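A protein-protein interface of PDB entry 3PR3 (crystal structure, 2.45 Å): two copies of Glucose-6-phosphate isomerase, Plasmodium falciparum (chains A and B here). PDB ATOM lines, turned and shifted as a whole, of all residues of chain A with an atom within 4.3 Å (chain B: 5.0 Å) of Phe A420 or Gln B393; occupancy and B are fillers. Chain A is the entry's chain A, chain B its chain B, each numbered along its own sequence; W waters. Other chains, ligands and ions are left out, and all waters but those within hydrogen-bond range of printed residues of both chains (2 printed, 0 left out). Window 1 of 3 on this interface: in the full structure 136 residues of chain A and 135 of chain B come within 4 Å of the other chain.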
ATOM      1  N   VAL A 376      16.813 -28.682  -1.233  1.00  0.00           N
ATOM      2  CA  VAL A 376      17.565 -27.921  -2.229  1.00  0.00           C
ATOM      3  C   VAL A 376      17.869 -26.569  -1.602  1.00  0.00           C
ATOM      4  O   VAL A 376      16.932 -25.863  -1.217  1.00  0.00           O
ATOM      5  CB  VAL A 376      16.851 -27.756  -3.615  1.00  0.00           C
ATOM      6  CG1 VAL A 376      17.685 -26.876  -4.568  1.00  0.00           C
ATOM      7  CG2 VAL A 376      16.563 -29.103  -4.270  1.00  0.00           C
ATOM      8  N   ALA A 377      19.156 -26.202  -1.510  1.00  0.00           N
ATOM      9  CA  ALA A 377      19.535 -24.868  -1.014  1.00  0.00           C
ATOM     10  C   ALA A 377      19.840 -23.989  -2.214  1.00  0.00           C
ATOM     11  O   ALA A 377      20.721 -24.320  -3.000  1.00  0.00           O
ATOM     12  CB  ALA A 377      20.737 -24.935  -0.067  1.00  0.00           C
ATOM     13  N   ILE A 378      19.057 -22.917  -2.394  1.00  0.00           N
ATOM     14  CA  ILE A 378      19.230 -21.929  -3.466  1.00  0.00           C
ATOM     15  C   ILE A 378      20.088 -20.837  -2.879  1.00  0.00           C
ATOM     16  O   ILE A 378      19.651 -20.108  -2.002  1.00  0.00           O
ATOM     17  CB  ILE A 378      17.879 -21.448  -4.073  1.00  0.00           C
ATOM     18  CG1 ILE A 378      17.095 -22.624  -4.751  1.00  0.00           C
ATOM     19  CG2 ILE A 378      18.068 -20.265  -5.029  1.00  0.00           C
ATOM     20  CD1 ILE A 378      17.789 -23.306  -6.000  1.00  0.00           C
ATOM     21  N   SER A 389      15.164 -16.875  -3.970  1.00  0.00           N
ATOM     22  CA  SER A 389      14.814 -18.104  -3.239  1.00  0.00           C
ATOM     23  C   SER A 389      13.320 -18.146  -2.858  1.00  0.00           C
ATOM     24  O   SER A 389      12.665 -19.179  -3.022  1.00  0.00           O
ATOM     25  CB  SER A 389      15.717 -18.263  -2.009  1.00  0.00           C
ATOM     26  OG  SER A 389      15.283 -19.255  -1.093  1.00  0.00           O
ATOM     27  N   GLN A 393      10.951 -21.021  -4.194  1.00  0.00           N
ATOM     28  CA  GLN A 393      10.207 -21.791  -3.203  1.00  0.00           C
ATOM     29  C   GLN A 393       8.785 -22.081  -3.708  1.00  0.00           C
ATOM     30  O   GLN A 393       8.387 -23.242  -3.708  1.00  0.00           O
ATOM     31  CB  GLN A 393      10.118 -21.025  -1.888  1.00  0.00           C
ATOM     32  CG  GLN A 393      11.063 -21.527  -0.820  1.00  0.00           C
ATOM     33  CD  GLN A 393      10.830 -20.902   0.535  1.00  0.00           C
ATOM     34  OE1 GLN A 393      10.150 -19.874   0.690  1.00  0.00           O
ATOM     35  NE2 GLN A 393      11.456 -21.485   1.540  1.00  0.00           N
ATOM     36  N   VAL A 418      12.295 -29.826  -0.155  1.00  0.00           N
ATOM     37  CA  VAL A 418      12.070 -28.604   0.597  1.00  0.00           C
ATOM     38  C   VAL A 418      13.128 -27.598   0.122  1.00  0.00           C
ATOM     39  O   VAL A 418      14.325 -27.881   0.195  1.00  0.00           O
ATOM     40  CB  VAL A 418      12.102 -28.804   2.135  1.00  0.00           C
ATOM     41  CG1 VAL A 418      12.157 -27.453   2.854  1.00  0.00           C
ATOM     42  CG2 VAL A 418      10.887 -29.620   2.594  1.00  0.00           C
ATOM     43  N   TYR A 419      12.677 -26.462  -0.411  1.00  0.00           N
ATOM     44  CA  TYR A 419      13.550 -25.398  -0.900  1.00  0.00           C
ATOM     45  C   TYR A 419      13.692 -24.295   0.130  1.00  0.00           C
ATOM     46  O   TYR A 419      12.724 -23.879   0.777  1.00  0.00           O
ATOM     47  CB  TYR A 419      12.995 -24.784  -2.191  1.00  0.00           C
ATOM     48  CG  TYR A 419      13.357 -25.533  -3.447  1.00  0.00           C
ATOM     49  CD1 TYR A 419      14.213 -24.976  -4.390  1.00  0.00           C
ATOM     50  CD2 TYR A 419      12.809 -26.788  -3.719  1.00  0.00           C
ATOM     51  CE1 TYR A 419      14.510 -25.644  -5.581  1.00  0.00           C
ATOM     52  CE2 TYR A 419      13.122 -27.476  -4.890  1.00  0.00           C
ATOM     53  CZ  TYR A 419      13.961 -26.892  -5.828  1.00  0.00           C
ATOM     54  OH  TYR A 419      14.236 -27.542  -7.006  1.00  0.00           O
ATOM     55  N   PHE A 420      14.916 -23.811   0.261  1.00  0.00           N
ATOM     56  CA  PHE A 420      15.294 -22.744   1.169  1.00  0.00           C
ATOM     57  C   PHE A 420      16.603 -22.161   0.655  1.00  0.00           C
ATOM     58  O   PHE A 420      17.149 -22.641  -0.338  1.00  0.00           O
ATOM     59  CB  PHE A 420      15.424 -23.283   2.627  1.00  0.00           C
ATOM     60  CG  PHE A 420      16.686 -24.057   2.923  1.00  0.00           C
ATOM     61  CD1 PHE A 420      17.710 -23.488   3.675  1.00  0.00           C
ATOM     62  CD2 PHE A 420      16.864 -25.345   2.426  1.00  0.00           C
ATOM     63  CE1 PHE A 420      18.885 -24.192   3.931  1.00  0.00           C
ATOM     64  CE2 PHE A 420      18.037 -26.050   2.685  1.00  0.00           C
ATOM     65  CZ  PHE A 420      19.039 -25.468   3.434  1.00  0.00           C
ATOM     66  N   GLY A 421      17.094 -21.146   1.350  1.00  0.00           N
ATOM     67  CA  GLY A 421      18.349 -20.490   1.027  1.00  0.00           C
ATOM     68  C   GLY A 421      18.333 -19.016   1.324  1.00  0.00           C
ATOM     69  O   GLY A 421      17.267 -18.398   1.459  1.00  0.00           O
ATOM     70  N   GLU A 422      19.541 -18.472   1.433  1.00  0.00           N
ATOM     71  CA  GLU A 422      19.864 -17.060   1.659  1.00  0.00           C
ATOM     72  C   GLU A 422      21.020 -16.712   0.714  1.00  0.00           C
ATOM     73  O   GLU A 422      21.790 -17.609   0.362  1.00  0.00           O
ATOM     74  CB  GLU A 422      20.318 -16.832   3.118  1.00  0.00           C
ATOM     75  CG  GLU A 422      19.169 -16.788   4.120  1.00  0.00           C
ATOM     76  CD  GLU A 422      18.180 -15.637   3.969  1.00  0.00           C
ATOM     77  OE1 GLU A 422      18.632 -14.470   3.897  1.00  0.00           O
ATOM     78  OE2 GLU A 422      16.955 -15.905   3.937  1.00  0.00           O
ATOM     79  N   SER A 430      25.310 -18.790   8.847  1.00  0.00           N
ATOM     80  CA  SER A 430      24.005 -19.124   9.375  1.00  0.00           C
ATOM     81  C   SER A 430      23.757 -20.625   9.474  1.00  0.00           C
ATOM     82  O   SER A 430      23.582 -21.151  10.568  1.00  0.00           O
ATOM     83  CB  SER A 430      22.913 -18.423   8.579  1.00  0.00           C
ATOM     84  OG  SER A 430      21.641 -18.840   9.030  1.00  0.00           O
ATOM     85  N   PHE A 431      23.743 -21.315   8.337  1.00  0.00           N
ATOM     86  CA  PHE A 431      23.372 -22.727   8.297  1.00  0.00           C
ATOM     87  C   PHE A 431      24.316 -23.611   7.499  1.00  0.00           C
ATOM     88  O   PHE A 431      23.991 -24.790   7.350  1.00  0.00           O
ATOM     89  CB  PHE A 431      21.918 -22.869   7.739  1.00  0.00           C
ATOM     90  CG  PHE A 431      21.692 -22.110   6.442  1.00  0.00           C
ATOM     91  CD1 PHE A 431      22.165 -22.607   5.229  1.00  0.00           C
ATOM     92  CD2 PHE A 431      21.033 -20.893   6.440  1.00  0.00           C
ATOM     93  CE1 PHE A 431      21.986 -21.887   4.042  1.00  0.00           C
ATOM     94  CE2 PHE A 431      20.834 -20.190   5.245  1.00  0.00           C
ATOM     95  CZ  PHE A 431      21.304 -20.697   4.059  1.00  0.00           C
ATOM     96  N   ILE A 441      22.727 -31.647   1.966  1.00  0.00           N
ATOM     97  CA  ILE A 441      21.762 -30.790   1.272  1.00  0.00           C
ATOM     98  C   ILE A 441      22.390 -30.316  -0.028  1.00  0.00           C
ATOM     99  O   ILE A 441      23.287 -29.465   0.034  1.00  0.00           O
ATOM    100  CB  ILE A 441      21.316 -29.600   2.174  1.00  0.00           C
ATOM    101  CG1 ILE A 441      20.547 -30.109   3.401  1.00  0.00           C
ATOM    102  CG2 ILE A 441      20.488 -28.552   1.391  1.00  0.00           C
ATOM    103  CD1 ILE A 441      20.859 -29.363   4.534  1.00  0.00           C
ATOM    104  N   SER B 389      12.460 -16.250  11.385  1.00  0.00           N
ATOM    105  CA  SER B 389      12.940 -17.541  10.850  1.00  0.00           C
ATOM    106  C   SER B 389      14.392 -17.501  10.390  1.00  0.00           C
ATOM    107  O   SER B 389      15.115 -18.464  10.634  1.00  0.00           O
ATOM    108  CB  SER B 389      12.029 -18.092   9.756  1.00  0.00           C
ATOM    109  OG  SER B 389      12.014 -17.230   8.633  1.00  0.00           O
ATOM    110  N   ALA B 390      14.844 -16.379   9.789  1.00  0.00           N
ATOM    111  CA  ALA B 390      16.254 -16.213   9.375  1.00  0.00           C
ATOM    112  C   ALA B 390      17.165 -16.344  10.615  1.00  0.00           C
ATOM    113  O   ALA B 390      18.255 -16.901  10.517  1.00  0.00           O
ATOM    114  CB  ALA B 390      16.455 -14.858   8.705  1.00  0.00           C
ATOM    115  N   HIS B 391      16.680 -15.879  11.787  1.00  0.00           N
ATOM    116  CA  HIS B 391      17.439 -15.970  13.031  1.00  0.00           C
ATOM    117  C   HIS B 391      17.413 -17.401  13.597  1.00  0.00           C
ATOM    118  O   HIS B 391      18.468 -17.941  13.950  1.00  0.00           O
ATOM    119  CB  HIS B 391      16.992 -14.904  14.065  1.00  0.00           C
ATOM    120  CG  HIS B 391      17.598 -15.137  15.412  1.00  0.00           C
ATOM    121  ND1 HIS B 391      18.978 -15.276  15.571  1.00  0.00           N
ATOM    122  CD2 HIS B 391      16.996 -15.362  16.605  1.00  0.00           C
ATOM    123  CE1 HIS B 391      19.161 -15.555  16.849  1.00  0.00           C
ATOM    124  NE2 HIS B 391      18.001 -15.617  17.513  1.00  0.00           N
ATOM    125  N   ILE B 392      16.203 -18.006  13.665  1.00  0.00           N
ATOM    126  CA  ILE B 392      15.982 -19.372  14.128  1.00  0.00           C
ATOM    127  C   ILE B 392      16.742 -20.376  13.271  1.00  0.00           C
ATOM    128  O   ILE B 392      17.187 -21.385  13.797  1.00  0.00           O
ATOM    129  CB  ILE B 392      14.462 -19.690  14.288  1.00  0.00           C
ATOM    130  CG1 ILE B 392      13.790 -18.735  15.309  1.00  0.00           C
ATOM    131  CG2 ILE B 392      14.190 -21.176  14.647  1.00  0.00           C
ATOM    132  CD1 ILE B 392      14.568 -18.476  16.650  1.00  0.00           C
ATOM    133  N   GLN B 393      16.928 -20.076  11.967  1.00  0.00           N
ATOM    134  CA  GLN B 393      17.721 -20.900  11.047  1.00  0.00           C
ATOM    135  C   GLN B 393      19.157 -21.057  11.567  1.00  0.00           C
ATOM    136  O   GLN B 393      19.625 -22.182  11.676  1.00  0.00           O
ATOM    137  CB  GLN B 393      17.760 -20.254   9.668  1.00  0.00           C
ATOM    138  CG  GLN B 393      16.847 -20.918   8.661  1.00  0.00           C
ATOM    139  CD  GLN B 393      17.019 -20.399   7.255  1.00  0.00           C
ATOM    140  OE1 GLN B 393      17.617 -19.347   6.994  1.00  0.00           O
ATOM    141  NE2 GLN B 393      16.422 -21.100   6.327  1.00  0.00           N
ATOM    142  N   GLN B 394      19.839 -19.938  11.924  1.00  0.00           N
ATOM    143  CA  GLN B 394      21.211 -20.002  12.455  1.00  0.00           C
ATOM    144  C   GLN B 394      21.263 -20.638  13.830  1.00  0.00           C
ATOM    145  O   GLN B 394      22.048 -21.562  14.059  1.00  0.00           O
ATOM    146  CB  GLN B 394      21.921 -18.644  12.481  1.00  0.00           C
ATOM    147  CG  GLN B 394      23.360 -18.807  13.023  1.00  0.00           C
ATOM    148  CD  GLN B 394      24.069 -17.523  13.296  1.00  0.00           C
ATOM    149  OE1 GLN B 394      23.486 -16.444  13.273  1.00  0.00           O
ATOM    150  NE2 GLN B 394      25.353 -17.618  13.589  1.00  0.00           N
ATOM    151  N   LEU B 395      20.418 -20.139  14.738  1.00  0.00           N
ATOM    152  CA  LEU B 395      20.309 -20.623  16.109  1.00  0.00           C
ATOM    153  C   LEU B 395      20.150 -22.136  16.149  1.00  0.00           C
ATOM    154  O   LEU B 395      20.796 -22.793  16.962  1.00  0.00           O
ATOM    155  CB  LEU B 395      19.155 -19.897  16.834  1.00  0.00           C
ATOM    156  CG  LEU B 395      18.815 -20.345  18.265  1.00  0.00           C
ATOM    157  CD1 LEU B 395      20.007 -20.169  19.223  1.00  0.00           C
ATOM    158  CD2 LEU B 395      17.585 -19.622  18.778  1.00  0.00           C
ATOM    159  N   SER B 396      19.329 -22.690  15.267  1.00  0.00           N
ATOM    160  CA  SER B 396      19.071 -24.124  15.266  1.00  0.00           C
ATOM    161  C   SER B 396      20.074 -24.930  14.456  1.00  0.00           C
ATOM    162  O   SER B 396      20.655 -25.886  14.984  1.00  0.00           O
ATOM    163  CB  SER B 396      17.651 -24.397  14.791  1.00  0.00           C
ATOM    164  OG  SER B 396      16.742 -23.566  15.500  1.00  0.00           O
ATOM    165  N   MET B 397      20.296 -24.537  13.186  1.00  0.00           N
ATOM    166  CA  MET B 397      21.147 -25.278  12.251  1.00  0.00           C
ATOM    167  C   MET B 397      22.646 -25.198  12.525  1.00  0.00           C
ATOM    168  O   MET B 397      23.344 -26.204  12.445  1.00  0.00           O
ATOM    169  CB  MET B 397      20.768 -24.965  10.782  1.00  0.00           C
ATOM    170  CG  MET B 397      19.301 -25.266  10.460  1.00  0.00           C
ATOM    171  SD  MET B 397      18.811 -24.700   8.821  1.00  0.00           S
ATOM    172  CE  MET B 397      19.481 -26.010   7.835  1.00  0.00           C
ATOM    173  N   GLU B 398      23.133 -24.022  12.898  1.00  0.00           N
ATOM    174  CA  GLU B 398      24.534 -23.895  13.240  1.00  0.00           C
ATOM    175  C   GLU B 398      24.813 -24.571  14.610  1.00  0.00           C
ATOM    176  O   GLU B 398      25.906 -25.108  14.800  1.00  0.00           O
ATOM    177  CB  GLU B 398      24.990 -22.434  13.214  1.00  0.00           C
ATOM    178  CG  GLU B 398      26.502 -22.303  13.151  1.00  0.00           C
ATOM    179  CD  GLU B 398      26.999 -20.904  12.864  1.00  0.00           C
ATOM    180  OE1 GLU B 398      26.816 -20.027  13.732  1.00  0.00           O
ATOM    181  OE2 GLU B 398      27.595 -20.687  11.784  1.00  0.00           O
ATOM    182  N   VAL B 418      16.184 -29.300   8.773  1.00  0.00           N
ATOM    183  CA  VAL B 418      16.329 -28.152   7.910  1.00  0.00           C
ATOM    184  C   VAL B 418      15.201 -27.181   8.306  1.00  0.00           C
ATOM    185  O   VAL B 418      14.027 -27.550   8.264  1.00  0.00           O
ATOM    186  CB  VAL B 418      16.306 -28.502   6.401  1.00  0.00           C
ATOM    187  CG1 VAL B 418      16.159 -27.232   5.553  1.00  0.00           C
ATOM    188  CG2 VAL B 418      17.561 -29.268   6.014  1.00  0.00           C
ATOM    189  N   TYR B 419      15.578 -25.967   8.728  1.00  0.00           N
ATOM    190  CA  TYR B 419      14.641 -24.922   9.115  1.00  0.00           C
ATOM    191  C   TYR B 419      14.417 -23.946   7.976  1.00  0.00           C
ATOM    192  O   TYR B 419      15.356 -23.541   7.284  1.00  0.00           O
ATOM    193  CB  TYR B 419      15.153 -24.157  10.329  1.00  0.00           C
ATOM    194  CG  TYR B 419      14.845 -24.805  11.657  1.00  0.00           C
ATOM    195  CD1 TYR B 419      13.954 -24.218  12.552  1.00  0.00           C
ATOM    196  CD2 TYR B 419      15.469 -25.996  12.040  1.00  0.00           C
ATOM    197  CE1 TYR B 419      13.698 -24.794  13.800  1.00  0.00           C
ATOM    198  CE2 TYR B 419      15.200 -26.591  13.273  1.00  0.00           C
ATOM    199  CZ  TYR B 419      14.322 -25.980  14.150  1.00  0.00           C
ATOM    200  OH  TYR B 419      14.110 -26.538  15.375  1.00  0.00           O
ATOM    201  N   PHE B 420      13.164 -23.561   7.801  1.00  0.00           N
ATOM    202  CA  PHE B 420      12.718 -22.611   6.790  1.00  0.00           C
ATOM    203  C   PHE B 420      11.361 -22.057   7.242  1.00  0.00           C
ATOM    204  O   PHE B 420      10.838 -22.464   8.267  1.00  0.00           O
ATOM    205  CB  PHE B 420      12.625 -23.296   5.395  1.00  0.00           C
ATOM    206  CG  PHE B 420      11.415 -24.174   5.187  1.00  0.00           C
ATOM    207  CD1 PHE B 420      10.357 -23.746   4.398  1.00  0.00           C
ATOM    208  CD2 PHE B 420      11.320 -25.411   5.806  1.00  0.00           C
ATOM    209  CE1 PHE B 420       9.224 -24.542   4.224  1.00  0.00           C
ATOM    210  CE2 PHE B 420      10.185 -26.206   5.639  1.00  0.00           C
ATOM    211  CZ  PHE B 420       9.146 -25.768   4.844  1.00  0.00           C
HETATM  212  O   HOH W   1      19.419 -17.630   8.178  1.00  0.00           O
HETATM  213  O   HOH W   2      15.197 -19.849   3.743  1.00  0.00           O
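Water W1 lies within hydrogen-bond range of the side-chain hydroxyl (OG) of Ser A430 (2.7 Å), the backbone carbonyl oxygen (O) of Ala B390 (2.7 Å) and the side-chain amide oxygen (OE1) of Gln B393 (2.8 Å).
Water W2 bridges the side-chain amide nitrogen (NE2) of Gln B393 and the backbone NH (N) of Gly A421.
NE2 of Gln B393 lies within hydrogen-bond range of O of Tyr B419 (2.8 Å).
The backbone carbonyl oxygen of Phe A420 lies within hydrogen-bond range of the backbone NH of Ile A378 (2.8 Å).
The side-chain amide nitrogen (NE2) of Gln A393 lies within hydrogen-bond range of the backbone carbonyl oxygen (O) of Tyr A419 (2.8 Å).
The backbone NH of Phe A420 sits at hydrogen-bond distance from the backbone carbonyl oxygen of Val A376.
The backbone NH of Val A376 lies within hydrogen-bond range of the backbone carbonyl oxygen of Val A418 (3.0 Å).
The side-chain amide nitrogen (NE2) of Gln B394 lies within hydrogen-bond range of the side-chain carboxylate (OE1) of Glu B398 (2.8 Å).
NE2 of Gln A393 touches CD1 of Phe B420, 3.8 Å away.
Val A418 touches Phe B420.
Gln B393 touches Phe A420.
CE2 of Phe A420 touches CG1 of Val B418, 3.6 Å away.
Phe A420 touches Phe B420 (CB to CB, 3.9 Å).
Ser A430 touches Gln B394.
CB of Glu B398 touches O of Ser A430, 3.3 Å away.
Gln B393 touches Phe A431 (OE1 to CE2, 3.8 Å).
CB of Phe A431 touches SD of Met B397, at 3.8 Å.
Ile A441 touches Val B418 (CD1 to CG2, 3.6 Å).
Hydrophobic or aromatic side chains of chain B within 4 Å of the printed part of chain A: Met B397, Val B418 and Phe B420.
Among the printed residues, no Asp or Glu carboxylate lies within 4 Å of a Lys or Arg side-chain nitrogen of the other chain.
Phe A420 touches just these residues of chain B: Gln B393, Val B418 and Phe B420.
Gln B393 touches just these residues of chain A: Phe A420 and Phe A431.
Of the printed residues of chain B, Ile A441 touches Val B418 (3.6 Å).
Of the printed residues of chain A, Gln B394 touches Ser A430.
Printed residues of chain B within 4 Å of Ser A430: Gln B394 and Glu B398.
Printed residues of chain A within 4 Å of Met B397: Phe A431 (3.8 Å).
Of the printed residues of chain B, Gln A393 touches Phe B420.
The nearest printed residue of chain A that does not touch Gln B394 is Phe A431 (5.0 Å).
Gln A393 touches Phe B420, and with the chains exchanged Phe A420 touches Gln B393.
Val A418 touches Phe B420, and with the chains exchanged Phe A420 touches Val B418.
Phe B420 touches its own counterpart, Phe A420.
Positions printed for both chains: 389, 393, 418, 419 and 420.
Of the 10 pairs that touch across the chains among the printed residues, 5 have their exchanged pair printed and touching as well.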
